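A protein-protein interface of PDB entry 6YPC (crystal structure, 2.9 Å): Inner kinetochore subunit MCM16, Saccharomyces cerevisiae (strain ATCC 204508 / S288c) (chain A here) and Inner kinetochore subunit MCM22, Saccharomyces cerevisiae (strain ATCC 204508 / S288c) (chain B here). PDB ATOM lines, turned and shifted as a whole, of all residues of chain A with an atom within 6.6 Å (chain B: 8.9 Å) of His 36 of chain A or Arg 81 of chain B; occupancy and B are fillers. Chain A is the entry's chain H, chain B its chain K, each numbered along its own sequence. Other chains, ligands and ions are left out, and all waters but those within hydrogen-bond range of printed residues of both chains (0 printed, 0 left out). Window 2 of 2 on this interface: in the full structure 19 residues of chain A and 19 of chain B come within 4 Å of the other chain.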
ATOM      1  N   MET A  30     -14.513 -19.300 -30.558  1.00  0.00           N
ATOM      2  CA  MET A  30     -13.565 -18.353 -31.131  1.00  0.00           C
ATOM      3  C   MET A  30     -14.192 -16.970 -31.262  1.00  0.00           C
ATOM      4  O   MET A  30     -13.635 -15.980 -30.772  1.00  0.00           O
ATOM      5  CB  MET A  30     -13.041 -18.869 -32.469  1.00  0.00           C
ATOM      6  CG  MET A  30     -12.325 -20.209 -32.349  1.00  0.00           C
ATOM      7  SD  MET A  30     -11.032 -20.476 -33.593  1.00  0.00           S
ATOM      8  CE  MET A  30      -9.942 -19.086 -33.292  1.00  0.00           C
ATOM      9  N   ILE A  31     -15.360 -16.882 -31.884  1.00  0.00           N
ATOM     10  CA  ILE A  31     -16.081 -15.616 -31.969  1.00  0.00           C
ATOM     11  C   ILE A  31     -16.037 -14.879 -30.630  1.00  0.00           C
ATOM     12  O   ILE A  31     -15.850 -13.657 -30.571  1.00  0.00           O
ATOM     13  CB  ILE A  31     -17.539 -15.857 -32.405  1.00  0.00           C
ATOM     14  CG1 ILE A  31     -17.613 -16.083 -33.910  1.00  0.00           C
ATOM     15  CG2 ILE A  31     -18.463 -14.727 -31.923  1.00  0.00           C
ATOM     16  CD1 ILE A  31     -18.829 -16.861 -34.319  1.00  0.00           C
ATOM     17  N   ALA A  32     -16.195 -15.602 -29.536  1.00  0.00           N
ATOM     18  CA  ALA A  32     -16.290 -14.851 -28.307  1.00  0.00           C
ATOM     19  C   ALA A  32     -14.911 -14.451 -27.818  1.00  0.00           C
ATOM     20  O   ALA A  32     -14.746 -13.344 -27.293  1.00  0.00           O
ATOM     21  CB  ALA A  32     -17.052 -15.652 -27.259  1.00  0.00           C
ATOM     22  N   LEU A  33     -13.916 -15.329 -27.978  1.00  0.00           N
ATOM     23  CA  LEU A  33     -12.539 -14.942 -27.681  1.00  0.00           C
ATOM     24  C   LEU A  33     -12.127 -13.736 -28.526  1.00  0.00           C
ATOM     25  O   LEU A  33     -11.645 -12.718 -28.008  1.00  0.00           O
ATOM     26  CB  LEU A  33     -11.602 -16.116 -27.944  1.00  0.00           C
ATOM     27  CG  LEU A  33     -11.791 -17.408 -27.128  1.00  0.00           C
ATOM     28  CD1 LEU A  33     -10.935 -18.568 -27.644  1.00  0.00           C
ATOM     29  CD2 LEU A  33     -11.516 -17.181 -25.648  1.00  0.00           C
ATOM     30  N   GLN A  34     -12.346 -13.819 -29.835  1.00  0.00           N
ATOM     31  CA  GLN A  34     -11.912 -12.746 -30.713  1.00  0.00           C
ATOM     32  C   GLN A  34     -12.539 -11.416 -30.320  1.00  0.00           C
ATOM     33  O   GLN A  34     -11.845 -10.400 -30.199  1.00  0.00           O
ATOM     34  CB  GLN A  34     -12.239 -13.111 -32.150  1.00  0.00           C
ATOM     35  CG  GLN A  34     -11.430 -14.290 -32.592  1.00  0.00           C
ATOM     36  CD  GLN A  34     -11.616 -14.614 -34.055  1.00  0.00           C
ATOM     37  OE1 GLN A  34     -12.425 -13.984 -34.751  1.00  0.00           O
ATOM     38  NE2 GLN A  34     -10.882 -15.617 -34.536  1.00  0.00           N
ATOM     39  N   ILE A  35     -13.847 -11.398 -30.113  1.00  0.00           N
ATOM     40  CA  ILE A  35     -14.521 -10.135 -29.848  1.00  0.00           C
ATOM     41  C   ILE A  35     -14.030  -9.531 -28.548  1.00  0.00           C
ATOM     42  O   ILE A  35     -13.736  -8.332 -28.467  1.00  0.00           O
ATOM     43  CB  ILE A  35     -16.034 -10.341 -29.806  1.00  0.00           C
ATOM     44  CG1 ILE A  35     -16.526 -10.662 -31.206  1.00  0.00           C
ATOM     45  CG2 ILE A  35     -16.707  -9.114 -29.149  1.00  0.00           C
ATOM     46  CD1 ILE A  35     -17.978 -10.412 -31.367  1.00  0.00           C
ATOM     47  N   HIS A  36     -13.951 -10.337 -27.513  1.00  0.00           N
ATOM     48  CA  HIS A  36     -13.711  -9.790 -26.197  1.00  0.00           C
ATOM     49  C   HIS A  36     -12.244  -9.742 -25.854  1.00  0.00           C
ATOM     50  O   HIS A  36     -11.902  -9.419 -24.713  1.00  0.00           O
ATOM     51  CB  HIS A  36     -14.461 -10.602 -25.156  1.00  0.00           C
ATOM     52  CG  HIS A  36     -15.941 -10.436 -25.240  1.00  0.00           C
ATOM     53  ND1 HIS A  36     -16.752 -11.315 -25.926  1.00  0.00           N
ATOM     54  CD2 HIS A  36     -16.759  -9.478 -24.738  1.00  0.00           C
ATOM     55  CE1 HIS A  36     -18.009 -10.913 -25.828  1.00  0.00           C
ATOM     56  NE2 HIS A  36     -18.042  -9.806 -25.106  1.00  0.00           N
ATOM     57  N   SER A  37     -11.372 -10.088 -26.793  1.00  0.00           N
ATOM     58  CA  SER A  37      -9.948  -9.836 -26.634  1.00  0.00           C
ATOM     59  C   SER A  37      -9.475  -8.763 -27.605  1.00  0.00           C
ATOM     60  O   SER A  37      -8.271  -8.648 -27.864  1.00  0.00           O
ATOM     61  CB  SER A  37      -9.138 -11.122 -26.805  1.00  0.00           C
ATOM     62  OG  SER A  37      -9.309 -11.698 -28.093  1.00  0.00           O
ATOM     63  N   GLY A  38     -10.412  -7.985 -28.151  1.00  0.00           N
ATOM     64  CA  GLY A  38     -10.073  -6.909 -29.052  1.00  0.00           C
ATOM     65  C   GLY A  38      -9.374  -7.326 -30.326  1.00  0.00           C
ATOM     66  O   GLY A  38      -8.707  -6.489 -30.944  1.00  0.00           O
ATOM     67  N   TYR A  39      -9.489  -8.597 -30.734  1.00  0.00           N
ATOM     68  CA  TYR A  39      -8.914  -9.033 -32.003  1.00  0.00           C
ATOM     69  C   TYR A  39      -9.497  -8.196 -33.121  1.00  0.00           C
ATOM     70  O   TYR A  39     -10.664  -7.808 -33.071  1.00  0.00           O
ATOM     71  CB  TYR A  39      -9.223 -10.498 -32.255  1.00  0.00           C
ATOM     72  CG  TYR A  39      -8.406 -11.205 -33.313  1.00  0.00           C
ATOM     73  CD1 TYR A  39      -7.034 -11.382 -33.172  1.00  0.00           C
ATOM     74  CD2 TYR A  39      -9.023 -11.767 -34.416  1.00  0.00           C
ATOM     75  CE1 TYR A  39      -6.292 -12.077 -34.138  1.00  0.00           C
ATOM     76  CE2 TYR A  39      -8.308 -12.457 -35.375  1.00  0.00           C
ATOM     77  CZ  TYR A  39      -6.944 -12.611 -35.238  1.00  0.00           C
ATOM     78  OH  TYR A  39      -6.239 -13.293 -36.217  1.00  0.00           O
ATOM     79  N   PHE B  26      -4.665 -19.222 -33.566  1.00  0.00           N
ATOM     80  CA  PHE B  26      -5.064 -17.965 -32.955  1.00  0.00           C
ATOM     81  C   PHE B  26      -4.519 -17.817 -31.548  1.00  0.00           C
ATOM     82  O   PHE B  26      -4.327 -16.693 -31.076  1.00  0.00           O
ATOM     83  CB  PHE B  26      -6.574 -17.881 -32.927  1.00  0.00           C
ATOM     84  CG  PHE B  26      -7.103 -16.953 -31.903  1.00  0.00           C
ATOM     85  CD1 PHE B  26      -7.242 -15.620 -32.185  1.00  0.00           C
ATOM     86  CD2 PHE B  26      -7.493 -17.415 -30.668  1.00  0.00           C
ATOM     87  CE1 PHE B  26      -7.749 -14.751 -31.262  1.00  0.00           C
ATOM     88  CE2 PHE B  26      -8.004 -16.552 -29.739  1.00  0.00           C
ATOM     89  CZ  PHE B  26      -8.136 -15.212 -30.033  1.00  0.00           C
ATOM     90  N   TYR B  30      -2.031 -14.858 -31.405  1.00  0.00           N
ATOM     91  CA  TYR B  30      -2.529 -13.603 -30.850  1.00  0.00           C
ATOM     92  C   TYR B  30      -2.787 -13.648 -29.358  1.00  0.00           C
ATOM     93  O   TYR B  30      -2.344 -12.750 -28.638  1.00  0.00           O
ATOM     94  CB  TYR B  30      -3.816 -13.193 -31.539  1.00  0.00           C
ATOM     95  CG  TYR B  30      -4.461 -11.959 -30.952  1.00  0.00           C
ATOM     96  CD1 TYR B  30      -4.140 -10.694 -31.414  1.00  0.00           C
ATOM     97  CD2 TYR B  30      -5.420 -12.059 -29.969  1.00  0.00           C
ATOM     98  CE1 TYR B  30      -4.751  -9.570 -30.889  1.00  0.00           C
ATOM     99  CE2 TYR B  30      -6.034 -10.939 -29.441  1.00  0.00           C
ATOM    100  CZ  TYR B  30      -5.696  -9.702 -29.901  1.00  0.00           C
ATOM    101  OH  TYR B  30      -6.311  -8.597 -29.359  1.00  0.00           O
ATOM    102  N   LEU B  31      -3.522 -14.644 -28.869  1.00  0.00           N
ATOM    103  CA  LEU B  31      -4.047 -14.540 -27.512  1.00  0.00           C
ATOM    104  C   LEU B  31      -2.967 -14.711 -26.462  1.00  0.00           C
ATOM    105  O   LEU B  31      -2.968 -14.005 -25.448  1.00  0.00           O
ATOM    106  CB  LEU B  31      -5.141 -15.562 -27.295  1.00  0.00           C
ATOM    107  CG  LEU B  31      -5.914 -15.266 -26.021  1.00  0.00           C
ATOM    108  CD1 LEU B  31      -6.523 -13.897 -26.104  1.00  0.00           C
ATOM    109  CD2 LEU B  31      -7.005 -16.305 -25.845  1.00  0.00           C
ATOM    110  N   ILE B  73      -4.794 -16.626 -15.632  1.00  0.00           N
ATOM    111  CA  ILE B  73      -6.036 -16.153 -15.031  1.00  0.00           C
ATOM    112  C   ILE B  73      -6.737 -15.087 -15.875  1.00  0.00           C
ATOM    113  O   ILE B  73      -7.974 -14.995 -15.799  1.00  0.00           O
ATOM    114  CB  ILE B  73      -5.785 -15.654 -13.599  1.00  0.00           C
ATOM    115  CG1 ILE B  73      -7.098 -15.386 -12.874  1.00  0.00           C
ATOM    116  CG2 ILE B  73      -4.969 -14.404 -13.593  1.00  0.00           C
ATOM    117  CD1 ILE B  73      -7.901 -16.632 -12.617  1.00  0.00           C
ATOM    118  N   PRO B  74      -6.048 -14.262 -16.692  1.00  0.00           N
ATOM    119  CA  PRO B  74      -6.824 -13.361 -17.562  1.00  0.00           C
ATOM    120  C   PRO B  74      -7.761 -14.111 -18.463  1.00  0.00           C
ATOM    121  O   PRO B  74      -8.907 -13.687 -18.625  1.00  0.00           O
ATOM    122  CB  PRO B  74      -5.757 -12.618 -18.371  1.00  0.00           C
ATOM    123  CG  PRO B  74      -4.566 -12.689 -17.556  1.00  0.00           C
ATOM    124  CD  PRO B  74      -4.605 -14.010 -16.865  1.00  0.00           C
ATOM    125  N   ILE B  75      -7.297 -15.221 -19.047  1.00  0.00           N
ATOM    126  CA  ILE B  75      -8.173 -16.078 -19.846  1.00  0.00           C
ATOM    127  C   ILE B  75      -9.495 -16.284 -19.128  1.00  0.00           C
ATOM    128  O   ILE B  75     -10.572 -15.954 -19.645  1.00  0.00           O
ATOM    129  CB  ILE B  75      -7.500 -17.427 -20.134  1.00  0.00           C
ATOM    130  CG1 ILE B  75      -6.238 -17.198 -20.925  1.00  0.00           C
ATOM    131  CG2 ILE B  75      -8.429 -18.276 -20.948  1.00  0.00           C
ATOM    132  CD1 ILE B  75      -6.525 -16.570 -22.257  1.00  0.00           C
ATOM    133  N   TYR B  76      -9.418 -16.832 -17.916  1.00  0.00           N
ATOM    134  CA  TYR B  76     -10.605 -16.985 -17.095  1.00  0.00           C
ATOM    135  C   TYR B  76     -11.401 -15.696 -17.067  1.00  0.00           C
ATOM    136  O   TYR B  76     -12.603 -15.699 -17.320  1.00  0.00           O
ATOM    137  CB  TYR B  76     -10.225 -17.399 -15.677  1.00  0.00           C
ATOM    138  CG  TYR B  76     -11.342 -17.092 -14.736  1.00  0.00           C
ATOM    139  CD1 TYR B  76     -12.498 -17.864 -14.735  1.00  0.00           C
ATOM    140  CD2 TYR B  76     -11.276 -15.995 -13.886  1.00  0.00           C
ATOM    141  CE1 TYR B  76     -13.547 -17.569 -13.896  1.00  0.00           C
ATOM    142  CE2 TYR B  76     -12.320 -15.687 -13.037  1.00  0.00           C
ATOM    143  CZ  TYR B  76     -13.454 -16.477 -13.040  1.00  0.00           C
ATOM    144  OH  TYR B  76     -14.499 -16.167 -12.197  1.00  0.00           O
ATOM    145  N   ARG B  77     -10.738 -14.571 -16.795  1.00  0.00           N
ATOM    146  CA  ARG B  77     -11.472 -13.309 -16.738  1.00  0.00           C
ATOM    147  C   ARG B  77     -12.080 -12.949 -18.083  1.00  0.00           C
ATOM    148  O   ARG B  77     -13.135 -12.301 -18.135  1.00  0.00           O
ATOM    149  CB  ARG B  77     -10.567 -12.188 -16.247  1.00  0.00           C
ATOM    150  CG  ARG B  77     -10.569 -12.117 -14.734  1.00  0.00           C
ATOM    151  CD  ARG B  77      -9.746 -10.970 -14.168  1.00  0.00           C
ATOM    152  NE  ARG B  77      -8.349 -11.083 -14.564  1.00  0.00           N
ATOM    153  CZ  ARG B  77      -7.369 -11.400 -13.729  1.00  0.00           C
ATOM    154  NH1 ARG B  77      -7.632 -11.640 -12.441  1.00  0.00           N
ATOM    155  NH2 ARG B  77      -6.128 -11.477 -14.189  1.00  0.00           N
ATOM    156  N   LEU B  78     -11.438 -13.365 -19.172  1.00  0.00           N
ATOM    157  CA  LEU B  78     -11.943 -13.061 -20.501  1.00  0.00           C
ATOM    158  C   LEU B  78     -13.211 -13.852 -20.778  1.00  0.00           C
ATOM    159  O   LEU B  78     -14.209 -13.304 -21.271  1.00  0.00           O
ATOM    160  CB  LEU B  78     -10.865 -13.372 -21.533  1.00  0.00           C
ATOM    161  CG  LEU B  78     -11.324 -13.596 -22.962  1.00  0.00           C
ATOM    162  CD1 LEU B  78     -11.626 -12.260 -23.576  1.00  0.00           C
ATOM    163  CD2 LEU B  78     -10.245 -14.324 -23.760  1.00  0.00           C
ATOM    164  N   LEU B  79     -13.189 -15.148 -20.453  1.00  0.00           N
ATOM    165  CA  LEU B  79     -14.394 -15.963 -20.553  1.00  0.00           C
ATOM    166  C   LEU B  79     -15.502 -15.384 -19.694  1.00  0.00           C
ATOM    167  O   LEU B  79     -16.651 -15.260 -20.138  1.00  0.00           O
ATOM    168  CB  LEU B  79     -14.089 -17.399 -20.137  1.00  0.00           C
ATOM    169  CG  LEU B  79     -12.879 -17.967 -20.878  1.00  0.00           C
ATOM    170  CD1 LEU B  79     -12.260 -19.142 -20.129  1.00  0.00           C
ATOM    171  CD2 LEU B  79     -13.304 -18.354 -22.267  1.00  0.00           C
ATOM    172  N   LEU B  80     -15.169 -14.988 -18.476  1.00  0.00           N
ATOM    173  CA  LEU B  80     -16.160 -14.383 -17.604  1.00  0.00           C
ATOM    174  C   LEU B  80     -16.810 -13.170 -18.273  1.00  0.00           C
ATOM    175  O   LEU B  80     -18.041 -13.062 -18.319  1.00  0.00           O
ATOM    176  CB  LEU B  80     -15.495 -14.010 -16.281  1.00  0.00           C
ATOM    177  CG  LEU B  80     -16.461 -13.599 -15.179  1.00  0.00           C
ATOM    178  CD1 LEU B  80     -17.308 -14.777 -14.836  1.00  0.00           C
ATOM    179  CD2 LEU B  80     -15.717 -13.105 -13.969  1.00  0.00           C
ATOM    180  N   ARG B  81     -15.999 -12.259 -18.822  1.00  0.00           N
ATOM    181  CA  ARG B  81     -16.549 -11.037 -19.404  1.00  0.00           C
ATOM    182  C   ARG B  81     -17.505 -11.353 -20.539  1.00  0.00           C
ATOM    183  O   ARG B  81     -18.615 -10.800 -20.603  1.00  0.00           O
ATOM    184  CB  ARG B  81     -15.427 -10.129 -19.906  1.00  0.00           C
ATOM    185  CG  ARG B  81     -15.084  -9.011 -18.953  1.00  0.00           C
ATOM    186  CD  ARG B  81     -14.024  -8.118 -19.511  1.00  0.00           C
ATOM    187  NE  ARG B  81     -12.837  -8.892 -19.821  1.00  0.00           N
ATOM    188  CZ  ARG B  81     -12.351  -9.035 -21.046  1.00  0.00           C
ATOM    189  NH1 ARG B  81     -12.958  -8.436 -22.071  1.00  0.00           N
ATOM    190  NH2 ARG B  81     -11.261  -9.778 -21.241  1.00  0.00           N
ATOM    191  N   ALA B  82     -17.083 -12.254 -21.439  1.00  0.00           N
ATOM    192  CA  ALA B  82     -17.865 -12.699 -22.592  1.00  0.00           C
ATOM    193  C   ALA B  82     -19.136 -13.445 -22.205  1.00  0.00           C
ATOM    194  O   ALA B  82     -19.972 -13.697 -23.080  1.00  0.00           O
ATOM    195  CB  ALA B  82     -17.009 -13.597 -23.490  1.00  0.00           C
ATOM    196  N   ASN B  83     -19.296 -13.809 -20.935  1.00  0.00           N
ATOM    197  CA  ASN B  83     -20.521 -14.438 -20.471  1.00  0.00           C
ATOM    198  C   ASN B  83     -20.729 -15.780 -21.141  1.00  0.00           C
ATOM    199  O   ASN B  83     -21.842 -16.095 -21.549  1.00  0.00           O
ATOM    200  CB  ASN B  83     -21.743 -13.552 -20.726  1.00  0.00           C
ATOM    201  CG  ASN B  83     -21.791 -12.362 -19.818  1.00  0.00           C
ATOM    202  OD1 ASN B  83     -21.514 -12.474 -18.616  1.00  0.00           O
ATOM    203  ND2 ASN B  83     -22.173 -11.211 -20.370  1.00  0.00           N
ATOM    204  N   ILE B  84     -19.661 -16.559 -21.288  1.00  0.00           N
ATOM    205  CA  ILE B  84     -19.768 -17.835 -21.980  1.00  0.00           C
ATOM    206  C   ILE B  84     -19.291 -18.995 -21.115  1.00  0.00           C
ATOM    207  O   ILE B  84     -19.007 -20.073 -21.624  1.00  0.00           O
ATOM    208  CB  ILE B  84     -19.027 -17.813 -23.329  1.00  0.00           C
ATOM    209  CG1 ILE B  84     -17.513 -17.819 -23.129  1.00  0.00           C
ATOM    210  CG2 ILE B  84     -19.433 -16.620 -24.133  1.00  0.00           C
ATOM    211  CD1 ILE B  84     -16.767 -18.526 -24.264  1.00  0.00           C
ATOM    212  N   ILE B  85     -19.200 -18.782 -19.805  1.00  0.00           N
ATOM    213  CA  ILE B  85     -18.920 -19.851 -18.858  1.00  0.00           C
ATOM    214  C   ILE B  85     -19.822 -19.683 -17.645  1.00  0.00           C
ATOM    215  O   ILE B  85     -20.277 -18.579 -17.325  1.00  0.00           O
ATOM    216  CB  ILE B  85     -17.452 -19.876 -18.404  1.00  0.00           C
ATOM    217  CG1 ILE B  85     -17.037 -18.511 -17.878  1.00  0.00           C
ATOM    218  CG2 ILE B  85     -16.547 -20.335 -19.519  1.00  0.00           C
ATOM    219  CD1 ILE B  85     -15.770 -18.585 -17.069  1.00  0.00           C
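The backbone NH of Tyr 39 of chain A is in hydrogen-bond range of the backbone carbonyl oxygen of Gln 34 of chain A, at 3.0 Å. O of Phe 26 of chain B sits at hydrogen-bond distance from N of Leu 31 of chain B, 3.1 Å away. The backbone carbonyl oxygen (O) of Leu 33 of chain A sits at hydrogen-bond distance from the side-chain hydroxyl (OG) of Ser 37 of chain A, at 2.6 Å. O of Ala 32 of chain A is in hydrogen-bond range of ND1 of His 36 of chain A (3.2 Å).
NH1 of Arg 81 of chain B is in hydrogen-bond range of O of His 36 of chain A (3.0 Å). The side-chain hydroxyl (OH) of Tyr 30 of chain B sits at hydrogen-bond distance from the backbone carbonyl oxygen (O) of Ser 37 of chain A, 2.5 Å away. OH of Tyr 30 of chain B lies within hydrogen-bond range of N of Tyr 39 of chain A, at 3.5 Å.
Among the printed residues, pairs that only touch across the chains: Met 30 of chain A with Phe 26 of chain B (3.6 Å), Leu 33 of chain A with Leu 78 of chain B (3.7 Å), Gln 34 of chain A with Phe 26 of chain B (3.9 Å), His 36 of chain A with Leu 78 of chain B (3.1 Å), His 36 of chain A with Ala 82 of chain B (3.3 Å), Ser 37 of chain A with Leu 31 of chain B (3.9 Å), Ser 37 of chain A with Leu 78 of chain B (3.9 Å), Gly 38 of chain A with Tyr 30 of chain B (3.5 Å) and Tyr 39 of chain A with Phe 26 of chain B (3.9 Å).
Printed residues of chain A that touch a printed residue of chain B: Met 30, Leu 33, Gln 34, His 36, Ser 37, Gly 38 and Tyr 39. Along chain B the printed residues that touch a printed residue of chain A span positions 26 to 82. Among the printed residues, 12 pairs touch across the chains. Among the printed residues, no Asp or Glu carboxylate lies within 4 Å of a Lys or Arg side-chain nitrogen of the other chain.
Of the printed residues of chain B, Met 30 of chain A touches Phe 26 (3.6 Å). His 36 of chain A touches three residues of chain B. Printed residues of chain B within 4 Å of Tyr 39 of chain A: Phe 26 and Tyr 30. Printed residues of chain A within 4 Å of Leu 78 of chain B: Leu 33 (3.7 Å), His 36 (3.1 Å) and Ser 37 (3.9 Å). Arg 81 of chain B touches just one residue of chain A: His 36 (3.0 Å). The nearest printed residue of chain A that does not touch Leu 31 of chain B is Leu 33 of chain A (4.6 Å).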
